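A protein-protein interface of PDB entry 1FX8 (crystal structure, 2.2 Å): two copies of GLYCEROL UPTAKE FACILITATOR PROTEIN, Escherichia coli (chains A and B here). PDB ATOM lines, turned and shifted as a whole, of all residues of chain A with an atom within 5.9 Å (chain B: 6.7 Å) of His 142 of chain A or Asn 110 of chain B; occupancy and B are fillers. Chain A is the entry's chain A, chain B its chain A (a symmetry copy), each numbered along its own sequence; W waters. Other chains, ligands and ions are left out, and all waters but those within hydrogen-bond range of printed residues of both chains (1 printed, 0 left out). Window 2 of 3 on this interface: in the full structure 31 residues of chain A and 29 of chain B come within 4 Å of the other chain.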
ATOM      1  N   ASN A 140     -28.243 -10.866  17.982  1.00  0.00           N
ATOM      2  CA  ASN A 140     -27.367 -11.695  17.175  1.00  0.00           C
ATOM      3  C   ASN A 140     -26.130 -11.951  18.043  1.00  0.00           C
ATOM      4  O   ASN A 140     -25.697 -11.080  18.797  1.00  0.00           O
ATOM      5  CB  ASN A 140     -26.978 -10.948  15.897  1.00  0.00           C
ATOM      6  CG  ASN A 140     -25.997 -11.722  15.040  1.00  0.00           C
ATOM      7  OD1 ASN A 140     -24.816 -11.832  15.374  1.00  0.00           O
ATOM      8  ND2 ASN A 140     -26.481 -12.273  13.927  1.00  0.00           N
ATOM      9  N   PRO A 141     -25.552 -13.153  17.953  1.00  0.00           N
ATOM     10  CA  PRO A 141     -24.364 -13.505  18.739  1.00  0.00           C
ATOM     11  C   PRO A 141     -23.197 -12.516  18.631  1.00  0.00           C
ATOM     12  O   PRO A 141     -22.466 -12.308  19.592  1.00  0.00           O
ATOM     13  CB  PRO A 141     -23.992 -14.883  18.197  1.00  0.00           C
ATOM     14  CG  PRO A 141     -25.315 -15.443  17.771  1.00  0.00           C
ATOM     15  CD  PRO A 141     -25.972 -14.275  17.099  1.00  0.00           C
ATOM     16  N   HIS A 142     -23.035 -11.895  17.470  1.00  0.00           N
ATOM     17  CA  HIS A 142     -21.924 -10.971  17.265  1.00  0.00           C
ATOM     18  C   HIS A 142     -22.100  -9.526  17.727  1.00  0.00           C
ATOM     19  O   HIS A 142     -21.208  -8.708  17.519  1.00  0.00           O
ATOM     20  CB  HIS A 142     -21.513 -10.970  15.790  1.00  0.00           C
ATOM     21  CG  HIS A 142     -21.192 -12.328  15.248  1.00  0.00           C
ATOM     22  ND1 HIS A 142     -22.132 -13.125  14.629  1.00  0.00           N
ATOM     23  CD2 HIS A 142     -20.032 -13.028  15.224  1.00  0.00           C
ATOM     24  CE1 HIS A 142     -21.565 -14.255  14.244  1.00  0.00           C
ATOM     25  NE2 HIS A 142     -20.291 -14.221  14.592  1.00  0.00           N
ATOM     26  N   ILE A 143     -23.228  -9.189  18.342  1.00  0.00           N
ATOM     27  CA  ILE A 143     -23.405  -7.815  18.802  1.00  0.00           C
ATOM     28  C   ILE A 143     -23.793  -7.748  20.269  1.00  0.00           C
ATOM     29  O   ILE A 143     -24.383  -8.682  20.799  1.00  0.00           O
ATOM     30  CB  ILE A 143     -24.456  -7.052  17.963  1.00  0.00           C
ATOM     31  CG1 ILE A 143     -25.847  -7.641  18.180  1.00  0.00           C
ATOM     32  CG2 ILE A 143     -24.076  -7.112  16.484  1.00  0.00           C
ATOM     33  CD1 ILE A 143     -26.935  -6.805  17.561  1.00  0.00           C
ATOM     34  N   ASN A 144     -23.452  -6.639  20.920  1.00  0.00           N
ATOM     35  CA  ASN A 144     -23.740  -6.461  22.337  1.00  0.00           C
ATOM     36  C   ASN A 144     -24.942  -5.564  22.612  1.00  0.00           C
ATOM     37  O   ASN A 144     -25.627  -5.119  21.689  1.00  0.00           O
ATOM     38  CB  ASN A 144     -22.511  -5.900  23.065  1.00  0.00           C
ATOM     39  CG  ASN A 144     -22.097  -4.531  22.549  1.00  0.00           C
ATOM     40  OD1 ASN A 144     -22.941  -3.714  22.170  1.00  0.00           O
ATOM     41  ND2 ASN A 144     -20.793  -4.268  22.552  1.00  0.00           N
ATOM     42  N   GLN A 147     -25.027  -2.019  20.944  1.00  0.00           N
ATOM     43  CA  GLN A 147     -25.173  -2.185  19.505  1.00  0.00           C
ATOM     44  C   GLN A 147     -26.605  -2.599  19.162  1.00  0.00           C
ATOM     45  O   GLN A 147     -27.186  -2.109  18.193  1.00  0.00           O
ATOM     46  CB  GLN A 147     -24.166  -3.221  19.008  1.00  0.00           C
ATOM     47  CG  GLN A 147     -22.735  -2.823  19.370  1.00  0.00           C
ATOM     48  CD  GLN A 147     -21.702  -3.884  19.052  1.00  0.00           C
ATOM     49  OE1 GLN A 147     -21.723  -4.989  19.606  1.00  0.00           O
ATOM     50  NE2 GLN A 147     -20.782  -3.549  18.156  1.00  0.00           N
ATOM     51  N   ARG A 228     -27.360 -13.196  28.528  1.00  0.00           N
ATOM     52  CA  ARG A 228     -26.351 -12.144  28.450  1.00  0.00           C
ATOM     53  C   ARG A 228     -26.188 -11.461  29.809  1.00  0.00           C
ATOM     54  O   ARG A 228     -27.105 -11.472  30.630  1.00  0.00           O
ATOM     55  CB  ARG A 228     -26.767 -11.114  27.395  1.00  0.00           C
ATOM     56  CG  ARG A 228     -27.248 -11.732  26.084  1.00  0.00           C
ATOM     57  CD  ARG A 228     -26.109 -12.220  25.208  1.00  0.00           C
ATOM     58  NE  ARG A 228     -25.361 -11.094  24.657  1.00  0.00           N
ATOM     59  CZ  ARG A 228     -25.124 -10.900  23.362  1.00  0.00           C
ATOM     60  NH1 ARG A 228     -25.569 -11.759  22.454  1.00  0.00           N
ATOM     61  NH2 ARG A 228     -24.451  -9.830  22.972  1.00  0.00           N
ATOM     62  N   VAL B  34     -22.974 -11.452   5.423  1.00  0.00           N
ATOM     63  CA  VAL B  34     -22.305 -11.652   6.706  1.00  0.00           C
ATOM     64  C   VAL B  34     -23.187 -12.144   7.848  1.00  0.00           C
ATOM     65  O   VAL B  34     -22.685 -12.460   8.921  1.00  0.00           O
ATOM     66  CB  VAL B  34     -21.606 -10.356   7.165  1.00  0.00           C
ATOM     67  CG1 VAL B  34     -20.580  -9.929   6.125  1.00  0.00           C
ATOM     68  CG2 VAL B  34     -22.644  -9.246   7.379  1.00  0.00           C
ATOM     69  N   TYR B 105     -23.146  -0.173   7.613  1.00  0.00           N
ATOM     70  CA  TYR B 105     -21.879  -0.770   8.015  1.00  0.00           C
ATOM     71  C   TYR B 105     -21.708  -0.644   9.530  1.00  0.00           C
ATOM     72  O   TYR B 105     -21.178  -1.542  10.185  1.00  0.00           O
ATOM     73  CB  TYR B 105     -20.713  -0.069   7.316  1.00  0.00           C
ATOM     74  CG  TYR B 105     -19.347  -0.499   7.812  1.00  0.00           C
ATOM     75  CD1 TYR B 105     -18.829  -1.756   7.488  1.00  0.00           C
ATOM     76  CD2 TYR B 105     -18.566   0.359   8.584  1.00  0.00           C
ATOM     77  CE1 TYR B 105     -17.560  -2.146   7.916  1.00  0.00           C
ATOM     78  CE2 TYR B 105     -17.296  -0.019   9.025  1.00  0.00           C
ATOM     79  CZ  TYR B 105     -16.802  -1.271   8.682  1.00  0.00           C
ATOM     80  OH  TYR B 105     -15.547  -1.642   9.096  1.00  0.00           O
ATOM     81  N   GLY B 106     -22.159   0.480  10.075  1.00  0.00           N
ATOM     82  CA  GLY B 106     -22.052   0.706  11.505  1.00  0.00           C
ATOM     83  C   GLY B 106     -22.894  -0.260  12.316  1.00  0.00           C
ATOM     84  O   GLY B 106     -22.490  -0.695  13.391  1.00  0.00           O
ATOM     85  N   LEU B 107     -24.069  -0.610  11.805  1.00  0.00           N
ATOM     86  CA  LEU B 107     -24.950  -1.532  12.513  1.00  0.00           C
ATOM     87  C   LEU B 107     -24.500  -2.983  12.371  1.00  0.00           C
ATOM     88  O   LEU B 107     -24.658  -3.773  13.299  1.00  0.00           O
ATOM     89  CB  LEU B 107     -26.386  -1.367  12.012  1.00  0.00           C
ATOM     90  CG  LEU B 107     -26.971   0.038  12.211  1.00  0.00           C
ATOM     91  CD1 LEU B 107     -28.319   0.137  11.523  1.00  0.00           C
ATOM     92  CD2 LEU B 107     -27.107   0.336  13.701  1.00  0.00           C
ATOM     93  N   TYR B 108     -23.937  -3.327  11.216  1.00  0.00           N
ATOM     94  CA  TYR B 108     -23.458  -4.688  10.958  1.00  0.00           C
ATOM     95  C   TYR B 108     -21.955  -4.837  11.226  1.00  0.00           C
ATOM     96  O   TYR B 108     -21.395  -5.912  11.033  1.00  0.00           O
ATOM     97  CB  TYR B 108     -23.730  -5.095   9.502  1.00  0.00           C
ATOM     98  CG  TYR B 108     -25.118  -5.632   9.217  1.00  0.00           C
ATOM     99  CD1 TYR B 108     -26.166  -4.782   8.861  1.00  0.00           C
ATOM    100  CD2 TYR B 108     -25.370  -7.004   9.263  1.00  0.00           C
ATOM    101  CE1 TYR B 108     -27.432  -5.290   8.551  1.00  0.00           C
ATOM    102  CE2 TYR B 108     -26.620  -7.520   8.958  1.00  0.00           C
ATOM    103  CZ  TYR B 108     -27.645  -6.662   8.602  1.00  0.00           C
ATOM    104  OH  TYR B 108     -28.876  -7.189   8.292  1.00  0.00           O
ATOM    105  N   TYR B 109     -21.319  -3.749  11.660  1.00  0.00           N
ATOM    106  CA  TYR B 109     -19.879  -3.696  11.954  1.00  0.00           C
ATOM    107  C   TYR B 109     -19.206  -5.002  12.391  1.00  0.00           C
ATOM    108  O   TYR B 109     -18.334  -5.520  11.696  1.00  0.00           O
ATOM    109  CB  TYR B 109     -19.616  -2.637  13.033  1.00  0.00           C
ATOM    110  CG  TYR B 109     -18.154  -2.367  13.290  1.00  0.00           C
ATOM    111  CD1 TYR B 109     -17.446  -1.459  12.500  1.00  0.00           C
ATOM    112  CD2 TYR B 109     -17.472  -3.020  14.320  1.00  0.00           C
ATOM    113  CE1 TYR B 109     -16.094  -1.202  12.727  1.00  0.00           C
ATOM    114  CE2 TYR B 109     -16.120  -2.775  14.556  1.00  0.00           C
ATOM    115  CZ  TYR B 109     -15.437  -1.863  13.757  1.00  0.00           C
ATOM    116  OH  TYR B 109     -14.103  -1.599  13.988  1.00  0.00           O
ATOM    117  N   ASN B 110     -19.601  -5.518  13.552  1.00  0.00           N
ATOM    118  CA  ASN B 110     -19.018  -6.739  14.093  1.00  0.00           C
ATOM    119  C   ASN B 110     -19.141  -7.959  13.195  1.00  0.00           C
ATOM    120  O   ASN B 110     -18.230  -8.789  13.145  1.00  0.00           O
ATOM    121  CB  ASN B 110     -19.625  -7.074  15.460  1.00  0.00           C
ATOM    122  CG  ASN B 110     -19.276  -6.048  16.529  1.00  0.00           C
ATOM    123  OD1 ASN B 110     -18.195  -5.471  16.524  1.00  0.00           O
ATOM    124  ND2 ASN B 110     -20.192  -5.833  17.462  1.00  0.00           N
ATOM    125  N   LEU B 111     -20.264  -8.084  12.493  1.00  0.00           N
ATOM    126  CA  LEU B 111     -20.455  -9.234  11.625  1.00  0.00           C
ATOM    127  C   LEU B 111     -19.476  -9.210  10.455  1.00  0.00           C
ATOM    128  O   LEU B 111     -19.039 -10.261   9.983  1.00  0.00           O
ATOM    129  CB  LEU B 111     -21.908  -9.306  11.133  1.00  0.00           C
ATOM    130  CG  LEU B 111     -22.913  -9.823  12.180  1.00  0.00           C
ATOM    131  CD1 LEU B 111     -23.203  -8.756  13.220  1.00  0.00           C
ATOM    132  CD2 LEU B 111     -24.208 -10.239  11.490  1.00  0.00           C
ATOM    133  N   PHE B 112     -19.117  -8.014   9.990  1.00  0.00           N
ATOM    134  CA  PHE B 112     -18.160  -7.906   8.894  1.00  0.00           C
ATOM    135  C   PHE B 112     -16.799  -8.436   9.321  1.00  0.00           C
ATOM    136  O   PHE B 112     -16.206  -9.266   8.630  1.00  0.00           O
ATOM    137  CB  PHE B 112     -18.001  -6.454   8.436  1.00  0.00           C
ATOM    138  CG  PHE B 112     -18.984  -6.043   7.388  1.00  0.00           C
ATOM    139  CD1 PHE B 112     -20.191  -5.446   7.738  1.00  0.00           C
ATOM    140  CD2 PHE B 112     -18.714  -6.274   6.045  1.00  0.00           C
ATOM    141  CE1 PHE B 112     -21.114  -5.087   6.763  1.00  0.00           C
ATOM    142  CE2 PHE B 112     -19.628  -5.921   5.061  1.00  0.00           C
ATOM    143  CZ  PHE B 112     -20.829  -5.326   5.420  1.00  0.00           C
ATOM    144  N   PHE B 113     -16.302  -7.965  10.461  1.00  0.00           N
ATOM    145  CA  PHE B 113     -15.000  -8.412  10.931  1.00  0.00           C
ATOM    146  C   PHE B 113     -14.959  -9.885  11.319  1.00  0.00           C
ATOM    147  O   PHE B 113     -13.975 -10.566  11.034  1.00  0.00           O
ATOM    148  CB  PHE B 113     -14.511  -7.540  12.093  1.00  0.00           C
ATOM    149  CG  PHE B 113     -14.070  -6.165  11.667  1.00  0.00           C
ATOM    150  CD1 PHE B 113     -14.991  -5.123  11.556  1.00  0.00           C
ATOM    151  CD2 PHE B 113     -12.739  -5.920  11.339  1.00  0.00           C
ATOM    152  CE1 PHE B 113     -14.594  -3.859  11.128  1.00  0.00           C
ATOM    153  CE2 PHE B 113     -12.328  -4.658  10.908  1.00  0.00           C
ATOM    154  CZ  PHE B 113     -13.257  -3.624  10.803  1.00  0.00           C
ATOM    155  N   ASP B 114     -16.017 -10.389  11.949  1.00  0.00           N
ATOM    156  CA  ASP B 114     -16.022 -11.794  12.334  1.00  0.00           C
ATOM    157  C   ASP B 114     -16.092 -12.695  11.105  1.00  0.00           C
ATOM    158  O   ASP B 114     -15.515 -13.780  11.092  1.00  0.00           O
ATOM    159  CB  ASP B 114     -17.172 -12.083  13.298  1.00  0.00           C
ATOM    160  CG  ASP B 114     -17.086 -11.240  14.566  1.00  0.00           C
ATOM    161  OD1 ASP B 114     -15.957 -10.961  15.029  1.00  0.00           O
ATOM    162  OD2 ASP B 114     -18.145 -10.860  15.112  1.00  0.00           O
ATOM    163  N   PHE B 115     -16.778 -12.239  10.061  1.00  0.00           N
ATOM    164  CA  PHE B 115     -16.872 -13.023   8.834  1.00  0.00           C
ATOM    165  C   PHE B 115     -15.500 -13.050   8.152  1.00  0.00           C
ATOM    166  O   PHE B 115     -15.022 -14.105   7.734  1.00  0.00           O
ATOM    167  CB  PHE B 115     -17.900 -12.413   7.878  1.00  0.00           C
ATOM    168  CG  PHE B 115     -18.140 -13.239   6.644  1.00  0.00           C
ATOM    169  CD1 PHE B 115     -19.162 -14.186   6.613  1.00  0.00           C
ATOM    170  CD2 PHE B 115     -17.340 -13.072   5.513  1.00  0.00           C
ATOM    171  CE1 PHE B 115     -19.388 -14.957   5.470  1.00  0.00           C
ATOM    172  CE2 PHE B 115     -17.548 -13.832   4.362  1.00  0.00           C
ATOM    173  CZ  PHE B 115     -18.576 -14.777   4.338  1.00  0.00           C
ATOM    174  N   THR B 118     -13.237 -15.260  10.235  1.00  0.00           N
ATOM    175  CA  THR B 118     -13.610 -16.662  10.098  1.00  0.00           C
ATOM    176  C   THR B 118     -13.210 -17.264   8.761  1.00  0.00           C
ATOM    177  O   THR B 118     -12.706 -18.384   8.708  1.00  0.00           O
ATOM    178  CB  THR B 118     -15.136 -16.843  10.289  1.00  0.00           C
ATOM    179  OG1 THR B 118     -15.473 -16.605  11.659  1.00  0.00           O
ATOM    180  CG2 THR B 118     -15.573 -18.245   9.906  1.00  0.00           C
HETATM  181  O   HOH W   1     -17.942 -15.151  12.882  1.00  0.00           O
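His 142 of chain A touches just these residues of chain B: Asn 110, Leu 111 and Asp 114.
Printed residues of chain A within 4 Å of Asn 110 of chain B: His 142 and Gln 147.
Of the printed residues of chain B, Asn 140 of chain A touches Leu 111 (3.9 Å).
Of the printed residues of chain B, Ile 143 of chain A touches Leu 111 (3.8 Å).
Of the printed residues of chain B, Gln 147 of chain A touches Asn 110 (2.5 Å).
Of the printed residues of chain A, Asp 114 of chain B touches His 142.
Printed residues of chain A within 4 Å of Leu 111 of chain B: Asn 140, His 142 and Ile 143.
The nearest residue of chain B that does not touch His 142 of chain A is Val 34 of chain B (5.7 Å).
The nearest printed residue of chain A that does not touch Asn 110 of chain B is Ile 143 of chain A (4.01 Å).
The nearest printed residue of chain B that does not touch Asn 140 of chain A is Val 34 of chain B (6.3 Å).
The backbone carbonyl oxygen of Asp 114 of chain B sits at hydrogen-bond distance from the side-chain hydroxyl of Thr 118 of chain B (2.9 Å).
O of Ile 143 of chain A sits at hydrogen-bond distance from NH2 of Arg 228 of chain A, at 2.5 Å.
N of Asn 144 of chain A sits at hydrogen-bond distance from OE1 of Gln 147 of chain A, at 2.7 Å.
The side-chain amide oxygen (OD1) of Asn 140 of chain A lies within hydrogen-bond range of the backbone NH (N) of His 142 of chain A (2.8 Å).
No position is printed for both chains.
Of the 6 pairs that touch across the chains among the printed residues, none has its exchanged pair printed and touching as well.
Hydrophobic or aromatic side chains of chain B that line the printed part of chain A: Leu 111.
Along chain A the printed residues that touch a printed residue of chain B span positions 140 to 147.
Among the printed residues, pairs that only touch across the chains: Asn 140 of chain A with Leu 111 of chain B (3.9 Å), His 142 of chain A with Leu 111 of chain B (3.8 Å), His 142 of chain A with Asp 114 of chain B (2.9 Å) and Ile 143 of chain A with Leu 111 of chain B (3.8 Å).
Water W1 lies within hydrogen-bond range of a ring nitrogen (NE2) of His 142 of chain A (3.1 Å), the side-chain hydroxyl of Thr 118 of chain B (3.1 Å) and the backbone carbonyl oxygen of Asp 114 of chain B (3.3 Å).
The side-chain amide nitrogen (NE2) of Gln 147 of chain A lies close to the side-chain amide nitrogen (ND2) of Asn 110 of chain B, at 2.5 Å.
ND2 of Asn 110 of chain B sits at hydrogen-bond distance from O of His 142 of chain A, 3.0 Å away.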
